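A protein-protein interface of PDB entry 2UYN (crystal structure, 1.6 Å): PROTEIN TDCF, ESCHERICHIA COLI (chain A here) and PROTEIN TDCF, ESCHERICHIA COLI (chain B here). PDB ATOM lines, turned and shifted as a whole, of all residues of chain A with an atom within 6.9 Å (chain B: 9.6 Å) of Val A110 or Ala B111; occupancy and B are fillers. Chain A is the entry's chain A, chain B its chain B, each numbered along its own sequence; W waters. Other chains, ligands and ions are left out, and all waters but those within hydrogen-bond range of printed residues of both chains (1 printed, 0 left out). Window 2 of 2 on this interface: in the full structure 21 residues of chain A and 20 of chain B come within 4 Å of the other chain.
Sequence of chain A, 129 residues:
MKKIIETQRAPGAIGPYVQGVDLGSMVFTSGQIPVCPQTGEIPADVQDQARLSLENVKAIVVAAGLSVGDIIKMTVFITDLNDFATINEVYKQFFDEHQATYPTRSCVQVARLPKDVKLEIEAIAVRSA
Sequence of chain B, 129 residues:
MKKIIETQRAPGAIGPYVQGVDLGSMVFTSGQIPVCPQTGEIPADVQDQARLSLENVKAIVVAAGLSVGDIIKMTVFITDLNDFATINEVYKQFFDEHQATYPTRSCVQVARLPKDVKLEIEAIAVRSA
Of the 14 printed residues of chain A, 4 touch a printed residue of chain B.
Among the printed residues, 9 pairs touch across the chains.
N of Val A108 lies within hydrogen-bond range of O of Val A76 (3.3 Å).
The backbone NH (N) of Ile A78 lies within hydrogen-bond range of the backbone carbonyl oxygen (O) of Val A108 (2.9 Å).
O of Ile A78 lies within hydrogen-bond range of N of Val A110 (2.8 Å).
N of Leu A81 sits at hydrogen-bond distance from OE1 of Gln A109 (2.9 Å).
The backbone carbonyl oxygen of Ile B78 lies within hydrogen-bond range of the backbone NH of Val B110, 2.8 Å away.
OD1 of Asp B116 lies within salt-bridge range of NE of Arg B112.
Printed residues of chain B within 4 Å of Leu A81: Arg B112 (3.6 Å), Leu B113 (3.5 Å) and Pro B114 (3.7 Å).
Gln A109 touches just these residues of chain B: Val B110, Ala B111 and Arg B112.
Val A110 touches just one residue of chain B: Ala B111 (3.97 Å).
Arg A112 touches none of the printed residues of chain B.
Val A117 touches none of the printed residues of chain B.
Of the printed residues of chain A, Phe B77 touches Val A108 (3.7 Å).
Printed residues of chain A within 4 Å of Val B110: Gln A109.
Of the printed residues of chain A, Arg B112 touches Leu A81 (3.6 Å) and Gln A109 (3.0 Å).
The nearest residue of chain B that does not touch Val A110 is Val B110 (4.7 Å).
Water W1 lies within hydrogen-bond range of OE1 of Gln A109 (2.7 Å), OD1 of Asp A80 (2.8 Å), NH1 of Arg B112 (2.8 Å) and N of Leu A81 (3.3 Å).
Among the printed residues, pairs that only touch across the chains: Gln A109 with Val B110 (3.3 Å), Leu A81 with Leu B113 (3.5 Å), Val A108 with Leu B113 (3.5 Å), Leu A81 with Arg B112 (3.6 Å), Val A108 with Phe B77 (3.7 Å), Leu A81 with Pro B114 (3.7 Å) and Val A110 with Ala B111 (3.97 Å).
N of Ala B111 lies within hydrogen-bond range of O of Gln A109, at 2.8 Å.
N of Gln A109 lies within hydrogen-bond range of O of Arg B112, at 3.0 Å.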
ATOM      1  N   VAL A  76       4.559 -34.595 -23.678  1.00  0.00           N
ATOM      2  CA  VAL A  76       4.200 -33.373 -24.391  1.00  0.00           C
ATOM      3  C   VAL A  76       5.001 -32.252 -23.724  1.00  0.00           C
ATOM      4  O   VAL A  76       4.672 -31.813 -22.588  1.00  0.00           O
ATOM      5  CB  VAL A  76       2.657 -33.112 -24.308  1.00  0.00           C
ATOM      6  CG1 VAL A  76       2.294 -31.876 -25.063  1.00  0.00           C
ATOM      7  CG2 VAL A  76       1.862 -34.357 -24.813  1.00  0.00           C
ATOM      8  N   PHE A  77       6.076 -31.808 -24.385  1.00  0.00           N
ATOM      9  CA  PHE A  77       6.851 -30.680 -23.855  1.00  0.00           C
ATOM     10  C   PHE A  77       6.233 -29.425 -24.465  1.00  0.00           C
ATOM     11  O   PHE A  77       6.026 -29.385 -25.666  1.00  0.00           O
ATOM     12  CB  PHE A  77       8.299 -30.750 -24.322  1.00  0.00           C
ATOM     13  CG  PHE A  77       9.012 -32.022 -23.926  1.00  0.00           C
ATOM     14  CD1 PHE A  77       9.521 -32.179 -22.644  1.00  0.00           C
ATOM     15  CD2 PHE A  77       9.216 -33.036 -24.892  1.00  0.00           C
ATOM     16  CE1 PHE A  77      10.215 -33.354 -22.284  1.00  0.00           C
ATOM     17  CE2 PHE A  77       9.896 -34.218 -24.536  1.00  0.00           C
ATOM     18  CZ  PHE A  77      10.416 -34.365 -23.230  1.00  0.00           C
ATOM     19  N   ILE A  78       5.929 -28.416 -23.652  1.00  0.00           N
ATOM     20  CA  ILE A  78       5.241 -27.228 -24.191  1.00  0.00           C
ATOM     21  C   ILE A  78       5.922 -25.967 -23.683  1.00  0.00           C
ATOM     22  O   ILE A  78       6.665 -26.027 -22.712  1.00  0.00           O
ATOM     23  CB  ILE A  78       3.741 -27.197 -23.824  1.00  0.00           C
ATOM     24  CG1 ILE A  78       3.499 -26.883 -22.335  1.00  0.00           C
ATOM     25  CG2 ILE A  78       3.054 -28.501 -24.253  1.00  0.00           C
ATOM     26  CD1 ILE A  78       1.964 -26.716 -21.977  1.00  0.00           C
ATOM     27  N   THR A  79       5.648 -24.836 -24.317  1.00  0.00           N
ATOM     28  CA  THR A  79       6.281 -23.590 -23.870  1.00  0.00           C
ATOM     29  C   THR A  79       5.377 -22.720 -22.996  1.00  0.00           C
ATOM     30  O   THR A  79       5.868 -21.736 -22.393  1.00  0.00           O
ATOM     31  CB  THR A  79       6.827 -22.753 -25.042  1.00  0.00           C
ATOM     32  OG1 THR A  79       5.749 -22.520 -25.956  1.00  0.00           O
ATOM     33  CG2 THR A  79       7.928 -23.493 -25.768  1.00  0.00           C
ATOM     34  N   ASP A  80       4.070 -23.045 -22.928  1.00  0.00           N
ATOM     35  CA  ASP A  80       3.174 -22.224 -22.125  1.00  0.00           C
ATOM     36  C   ASP A  80       1.970 -23.020 -21.622  1.00  0.00           C
ATOM     37  O   ASP A  80       1.070 -23.321 -22.398  1.00  0.00           O
ATOM     38  CB  ASP A  80       2.727 -20.982 -22.934  1.00  0.00           C
ATOM     39  CG  ASP A  80       1.908 -19.971 -22.090  1.00  0.00           C
ATOM     40  OD1 ASP A  80       1.605 -20.254 -20.904  1.00  0.00           O
ATOM     41  OD2 ASP A  80       1.595 -18.881 -22.618  1.00  0.00           O
ATOM     42  N   LEU A  81       1.944 -23.309 -20.319  1.00  0.00           N
ATOM     43  CA  LEU A  81       0.821 -24.028 -19.724  1.00  0.00           C
ATOM     44  C   LEU A  81      -0.520 -23.320 -19.844  1.00  0.00           C
ATOM     45  O   LEU A  81      -1.554 -23.956 -19.699  1.00  0.00           O
ATOM     46  CB  LEU A  81       1.119 -24.426 -18.269  1.00  0.00           C
ATOM     47  CG  LEU A  81       1.910 -25.737 -18.247  1.00  0.00           C
ATOM     48  CD1 LEU A  81       2.688 -25.867 -16.942  1.00  0.00           C
ATOM     49  CD2 LEU A  81       0.935 -26.945 -18.418  1.00  0.00           C
ATOM     50  N   VAL A 108       4.918 -31.010 -19.441  1.00  0.00           N
ATOM     51  CA  VAL A 108       5.675 -30.010 -18.666  1.00  0.00           C
ATOM     52  C   VAL A 108       5.961 -28.792 -19.513  1.00  0.00           C
ATOM     53  O   VAL A 108       6.110 -28.906 -20.750  1.00  0.00           O
ATOM     54  CB  VAL A 108       7.026 -30.611 -18.168  1.00  0.00           C
ATOM     55  CG1 VAL A 108       6.765 -31.888 -17.345  1.00  0.00           C
ATOM     56  CG2 VAL A 108       7.961 -30.915 -19.352  1.00  0.00           C
ATOM     57  N   GLN A 109       6.096 -27.638 -18.856  1.00  0.00           N
ATOM     58  CA  GLN A 109       6.442 -26.415 -19.594  1.00  0.00           C
ATOM     59  C   GLN A 109       7.952 -26.223 -19.554  1.00  0.00           C
ATOM     60  O   GLN A 109       8.514 -25.997 -18.487  1.00  0.00           O
ATOM     61  CB  GLN A 109       5.743 -25.196 -19.011  1.00  0.00           C
ATOM     62  CG  GLN A 109       6.074 -23.929 -19.786  1.00  0.00           C
ATOM     63  CD  GLN A 109       5.474 -22.707 -19.118  1.00  0.00           C
ATOM     64  OE1 GLN A 109       4.292 -22.716 -18.732  1.00  0.00           O
ATOM     65  NE2 GLN A 109       6.293 -21.660 -18.937  1.00  0.00           N
ATOM     66  N   VAL A 110       8.591 -26.379 -20.705  1.00  0.00           N
ATOM     67  CA  VAL A 110      10.037 -26.156 -20.842  1.00  0.00           C
ATOM     68  C   VAL A 110      10.315 -24.662 -21.166  1.00  0.00           C
ATOM     69  O   VAL A 110       9.362 -23.862 -21.324  1.00  0.00           O
ATOM     70  CB  VAL A 110      10.630 -27.099 -21.945  1.00  0.00           C
ATOM     71  CG1 VAL A 110      10.363 -28.544 -21.572  1.00  0.00           C
ATOM     72  CG2 VAL A 110      10.016 -26.791 -23.321  1.00  0.00           C
ATOM     73  N   ALA A 111      11.589 -24.268 -21.252  1.00  0.00           N
ATOM     74  CA  ALA A 111      11.919 -22.875 -21.610  1.00  0.00           C
ATOM     75  C   ALA A 111      11.719 -22.558 -23.091  1.00  0.00           C
ATOM     76  O   ALA A 111      11.240 -21.479 -23.464  1.00  0.00           O
ATOM     77  CB  ALA A 111      13.342 -22.546 -21.236  1.00  0.00           C
ATOM     78  N   ARG A 112      12.126 -23.478 -23.939  1.00  0.00           N
ATOM     79  CA  ARG A 112      12.142 -23.222 -25.387  1.00  0.00           C
ATOM     80  C   ARG A 112      12.293 -24.546 -26.101  1.00  0.00           C
ATOM     81  O   ARG A 112      12.768 -25.520 -25.507  1.00  0.00           O
ATOM     82  CB  ARG A 112      13.327 -22.292 -25.717  1.00  0.00           C
ATOM     83  CG  ARG A 112      13.174 -21.517 -27.006  1.00  0.00           C
ATOM     84  CD  ARG A 112      14.316 -20.479 -27.117  1.00  0.00           C
ATOM     85  NE  ARG A 112      14.199 -19.808 -28.410  1.00  0.00           N
ATOM     86  CZ  ARG A 112      15.146 -19.021 -28.913  1.00  0.00           C
ATOM     87  NH1 ARG A 112      16.280 -18.877 -28.237  1.00  0.00           N
ATOM     88  NH2 ARG A 112      14.970 -18.428 -30.108  1.00  0.00           N
ATOM     89  N   LEU A 113      11.881 -24.573 -27.368  1.00  0.00           N
ATOM     90  CA  LEU A 113      11.960 -25.789 -28.174  1.00  0.00           C
ATOM     91  C   LEU A 113      12.654 -25.510 -29.513  1.00  0.00           C
ATOM     92  O   LEU A 113      12.704 -24.355 -29.987  1.00  0.00           O
ATOM     93  CB  LEU A 113      10.530 -26.347 -28.393  1.00  0.00           C
ATOM     94  CG  LEU A 113       9.842 -26.904 -27.134  1.00  0.00           C
ATOM     95  CD1 LEU A 113       8.353 -27.101 -27.381  1.00  0.00           C
ATOM     96  CD2 LEU A 113      10.481 -28.219 -26.669  1.00  0.00           C
ATOM     97  N   VAL A 117       8.981 -23.672 -31.667  1.00  0.00           N
ATOM     98  CA  VAL A 117       7.608 -24.192 -31.642  1.00  0.00           C
ATOM     99  C   VAL A 117       7.010 -24.199 -30.231  1.00  0.00           C
ATOM    100  O   VAL A 117       7.732 -24.145 -29.242  1.00  0.00           O
ATOM    101  CB  VAL A 117       7.549 -25.598 -32.230  1.00  0.00           C
ATOM    102  CG1 VAL A 117       7.982 -25.553 -33.724  1.00  0.00           C
ATOM    103  CG2 VAL A 117       8.428 -26.569 -31.425  1.00  0.00           C
ATOM    104  N   LYS A 118       5.687 -24.312 -30.149  1.00  0.00           N
ATOM    105  CA  LYS A 118       4.988 -24.267 -28.861  1.00  0.00           C
ATOM    106  C   LYS A 118       4.911 -25.635 -28.151  1.00  0.00           C
ATOM    107  O   LYS A 118       4.603 -25.699 -26.951  1.00  0.00           O
ATOM    108  CB  LYS A 118       3.574 -23.714 -29.028  1.00  0.00           C
ATOM    109  CG  LYS A 118       3.560 -22.271 -29.493  1.00  0.00           C
ATOM    110  CD  LYS A 118       2.125 -21.861 -29.775  1.00  0.00           C
ATOM    111  CE  LYS A 118       2.058 -20.412 -30.308  1.00  0.00           C
ATOM    112  NZ  LYS A 118       2.534 -19.379 -29.313  1.00  0.00           N
ATOM    113  N   PHE B  77      10.806 -34.090 -13.048  1.00  0.00           N
ATOM    114  CA  PHE B  77      10.797 -32.691 -13.533  1.00  0.00           C
ATOM    115  C   PHE B  77      10.541 -31.795 -12.347  1.00  0.00           C
ATOM    116  O   PHE B  77       9.577 -32.022 -11.612  1.00  0.00           O
ATOM    117  CB  PHE B  77       9.657 -32.485 -14.513  1.00  0.00           C
ATOM    118  CG  PHE B  77       9.699 -33.414 -15.712  1.00  0.00           C
ATOM    119  CD1 PHE B  77      10.577 -33.176 -16.788  1.00  0.00           C
ATOM    120  CD2 PHE B  77       8.809 -34.505 -15.777  1.00  0.00           C
ATOM    121  CE1 PHE B  77      10.573 -34.025 -17.933  1.00  0.00           C
ATOM    122  CE2 PHE B  77       8.801 -35.356 -16.913  1.00  0.00           C
ATOM    123  CZ  PHE B  77       9.688 -35.108 -17.969  1.00  0.00           C
ATOM    124  N   ILE B  78      11.369 -30.770 -12.166  1.00  0.00           N
ATOM    125  CA  ILE B  78      11.180 -29.911 -10.997  1.00  0.00           C
ATOM    126  C   ILE B  78      11.183 -28.443 -11.411  1.00  0.00           C
ATOM    127  O   ILE B  78      11.665 -28.127 -12.492  1.00  0.00           O
ATOM    128  CB  ILE B  78      12.240 -30.169  -9.892  1.00  0.00           C
ATOM    129  CG1 ILE B  78      13.637 -29.723 -10.359  1.00  0.00           C
ATOM    130  CG2 ILE B  78      12.217 -31.609  -9.482  1.00  0.00           C
ATOM    131  CD1 ILE B  78      14.712 -29.896  -9.214  1.00  0.00           C
ATOM    132  N   THR B  79      10.682 -27.541 -10.552  1.00  0.00           N
ATOM    133  CA  THR B  79      10.732 -26.121 -10.948  1.00  0.00           C
ATOM    134  C   THR B  79      11.859 -25.329 -10.276  1.00  0.00           C
ATOM    135  O   THR B  79      12.118 -24.172 -10.663  1.00  0.00           O
ATOM    136  CB  THR B  79       9.375 -25.423 -10.687  1.00  0.00           C
ATOM    137  OG1 THR B  79       8.990 -25.648  -9.330  1.00  0.00           O
ATOM    138  CG2 THR B  79       8.295 -25.954 -11.609  1.00  0.00           C
ATOM    139  N   ASP B  80      12.552 -25.924  -9.304  1.00  0.00           N
ATOM    140  CA  ASP B  80      13.677 -25.216  -8.663  1.00  0.00           C
ATOM    141  C   ASP B  80      14.753 -26.167  -8.152  1.00  0.00           C
ATOM    142  O   ASP B  80      14.547 -26.851  -7.158  1.00  0.00           O
ATOM    143  CB  ASP B  80      13.118 -24.373  -7.505  1.00  0.00           C
ATOM    144  CG  ASP B  80      14.121 -23.369  -6.959  1.00  0.00           C
ATOM    145  OD1 ASP B  80      15.316 -23.499  -7.292  1.00  0.00           O
ATOM    146  OD2 ASP B  80      13.699 -22.436  -6.214  1.00  0.00           O
ATOM    147  N   VAL B 108      15.575 -32.666 -14.125  1.00  0.00           N
ATOM    148  CA  VAL B 108      15.821 -31.420 -14.836  1.00  0.00           C
ATOM    149  C   VAL B 108      14.892 -30.347 -14.281  1.00  0.00           C
ATOM    150  O   VAL B 108      13.787 -30.668 -13.808  1.00  0.00           O
ATOM    151  CB  VAL B 108      15.631 -31.545 -16.382  1.00  0.00           C
ATOM    152  CG1 VAL B 108      16.493 -32.663 -16.924  1.00  0.00           C
ATOM    153  CG2 VAL B 108      14.191 -31.783 -16.758  1.00  0.00           C
ATOM    154  N   GLN B 109      15.328 -29.092 -14.339  1.00  0.00           N
ATOM    155  CA  GLN B 109      14.456 -27.991 -13.912  1.00  0.00           C
ATOM    156  C   GLN B 109      13.730 -27.429 -15.098  1.00  0.00           C
ATOM    157  O   GLN B 109      14.344 -26.871 -16.000  1.00  0.00           O
ATOM    158  CB  GLN B 109      15.256 -26.899 -13.191  1.00  0.00           C
ATOM    159  CG  GLN B 109      14.360 -25.724 -12.712  1.00  0.00           C
ATOM    160  CD  GLN B 109      15.193 -24.596 -12.116  1.00  0.00           C
ATOM    161  OE1 GLN B 109      16.093 -24.840 -11.313  1.00  0.00           O
ATOM    162  NE2 GLN B 109      14.932 -23.359 -12.559  1.00  0.00           N
ATOM    163  N   VAL B 110      12.413 -27.607 -15.115  1.00  0.00           N
ATOM    164  CA  VAL B 110      11.577 -27.026 -16.177  1.00  0.00           C
ATOM    165  C   VAL B 110      11.099 -25.654 -15.753  1.00  0.00           C
ATOM    166  O   VAL B 110      11.431 -25.191 -14.648  1.00  0.00           O
ATOM    167  CB  VAL B 110      10.382 -27.943 -16.506  1.00  0.00           C
ATOM    168  CG1 VAL B 110      10.895 -29.280 -17.009  1.00  0.00           C
ATOM    169  CG2 VAL B 110       9.475 -28.131 -15.276  1.00  0.00           C
ATOM    170  N   ALA B 111      10.371 -24.971 -16.633  1.00  0.00           N
ATOM    171  CA  ALA B 111       9.860 -23.641 -16.274  1.00  0.00           C
ATOM    172  C   ALA B 111       8.638 -23.674 -15.350  1.00  0.00           C
ATOM    173  O   ALA B 111       8.547 -22.888 -14.399  1.00  0.00           O
ATOM    174  CB  ALA B 111       9.564 -22.830 -17.495  1.00  0.00           C
ATOM    175  N   ARG B 112       7.701 -24.576 -15.641  1.00  0.00           N
ATOM    176  CA  ARG B 112       6.418 -24.601 -14.939  1.00  0.00           C
ATOM    177  C   ARG B 112       5.805 -25.992 -15.073  1.00  0.00           C
ATOM    178  O   ARG B 112       6.063 -26.693 -16.049  1.00  0.00           O
ATOM    179  CB  ARG B 112       5.482 -23.527 -15.512  1.00  0.00           C
ATOM    180  CG  ARG B 112       4.257 -23.254 -14.614  1.00  0.00           C
ATOM    181  CD  ARG B 112       3.311 -22.237 -15.298  1.00  0.00           C
ATOM    182  NE  ARG B 112       2.285 -21.808 -14.356  1.00  0.00           N
ATOM    183  CZ  ARG B 112       1.249 -21.012 -14.644  1.00  0.00           C
ATOM    184  NH1 ARG B 112       1.061 -20.564 -15.885  1.00  0.00           N
ATOM    185  NH2 ARG B 112       0.384 -20.665 -13.674  1.00  0.00           N
ATOM    186  N   LEU B 113       5.006 -26.380 -14.080  1.00  0.00           N
ATOM    187  CA  LEU B 113       4.336 -27.670 -14.095  1.00  0.00           C
ATOM    188  C   LEU B 113       2.827 -27.477 -13.893  1.00  0.00           C
ATOM    189  O   LEU B 113       2.378 -26.448 -13.359  1.00  0.00           O
ATOM    190  CB  LEU B 113       4.900 -28.588 -12.982  1.00  0.00           C
ATOM    191  CG  LEU B 113       6.330 -29.024 -13.246  1.00  0.00           C
ATOM    192  CD1 LEU B 113       6.886 -29.690 -12.001  1.00  0.00           C
ATOM    193  CD2 LEU B 113       6.399 -29.977 -14.443  1.00  0.00           C
ATOM    194  N   PRO B 114       2.032 -28.459 -14.315  1.00  0.00           N
ATOM    195  CA  PRO B 114       0.581 -28.382 -14.102  1.00  0.00           C
ATOM    196  C   PRO B 114       0.223 -28.019 -12.645  1.00  0.00           C
ATOM    197  O   PRO B 114       0.827 -28.503 -11.689  1.00  0.00           O
ATOM    198  CB  PRO B 114       0.114 -29.791 -14.486  1.00  0.00           C
ATOM    199  CG  PRO B 114       1.118 -30.192 -15.576  1.00  0.00           C
ATOM    200  CD  PRO B 114       2.421 -29.698 -15.012  1.00  0.00           C
ATOM    201  N   ASP B 116       0.962 -25.604 -10.976  1.00  0.00           N
ATOM    202  CA  ASP B 116       2.058 -24.901 -10.311  1.00  0.00           C
ATOM    203  C   ASP B 116       2.715 -25.713  -9.197  1.00  0.00           C
ATOM    204  O   ASP B 116       3.268 -25.164  -8.224  1.00  0.00           O
ATOM    205  CB  ASP B 116       1.598 -23.514  -9.839  1.00  0.00           C
ATOM    206  CG  ASP B 116       1.538 -22.533 -10.996  1.00  0.00           C
ATOM    207  OD1 ASP B 116       2.577 -22.381 -11.677  1.00  0.00           O
ATOM    208  OD2 ASP B 116       0.465 -21.973 -11.241  1.00  0.00           O
ATOM    209  N   VAL B 117       2.676 -27.031  -9.341  1.00  0.00           N
ATOM    210  CA  VAL B 117       3.401 -27.884  -8.401  1.00  0.00           C
ATOM    211  C   VAL B 117       4.918 -27.737  -8.581  1.00  0.00           C
ATOM    212  O   VAL B 117       5.411 -27.194  -9.585  1.00  0.00           O
ATOM    213  CB  VAL B 117       2.979 -29.346  -8.553  1.00  0.00           C
ATOM    214  CG1 VAL B 117       1.466 -29.477  -8.295  1.00  0.00           C
ATOM    215  CG2 VAL B 117       3.349 -29.909  -9.953  1.00  0.00           C
ATOM    216  N   LYS B 118       5.660 -28.252  -7.614  1.00  0.00           N
ATOM    217  CA  LYS B 118       7.111 -28.091  -7.631  1.00  0.00           C
ATOM    218  C   LYS B 118       7.847 -29.258  -8.291  1.00  0.00           C
ATOM    219  O   LYS B 118       9.040 -29.149  -8.552  1.00  0.00           O
ATOM    220  CB  LYS B 118       7.631 -27.938  -6.206  1.00  0.00           C
ATOM    221  CG  LYS B 118       7.153 -26.674  -5.488  1.00  0.00           C
ATOM    222  CD  LYS B 118       7.591 -26.763  -4.034  1.00  0.00           C
ATOM    223  CE  LYS B 118       7.006 -25.591  -3.209  1.00  0.00           C
ATOM    224  NZ  LYS B 118       7.608 -24.330  -3.644  1.00  0.00           N
HETATM  225  O   HOH W   1       2.571 -20.728 -18.281  1.00  0.00           O
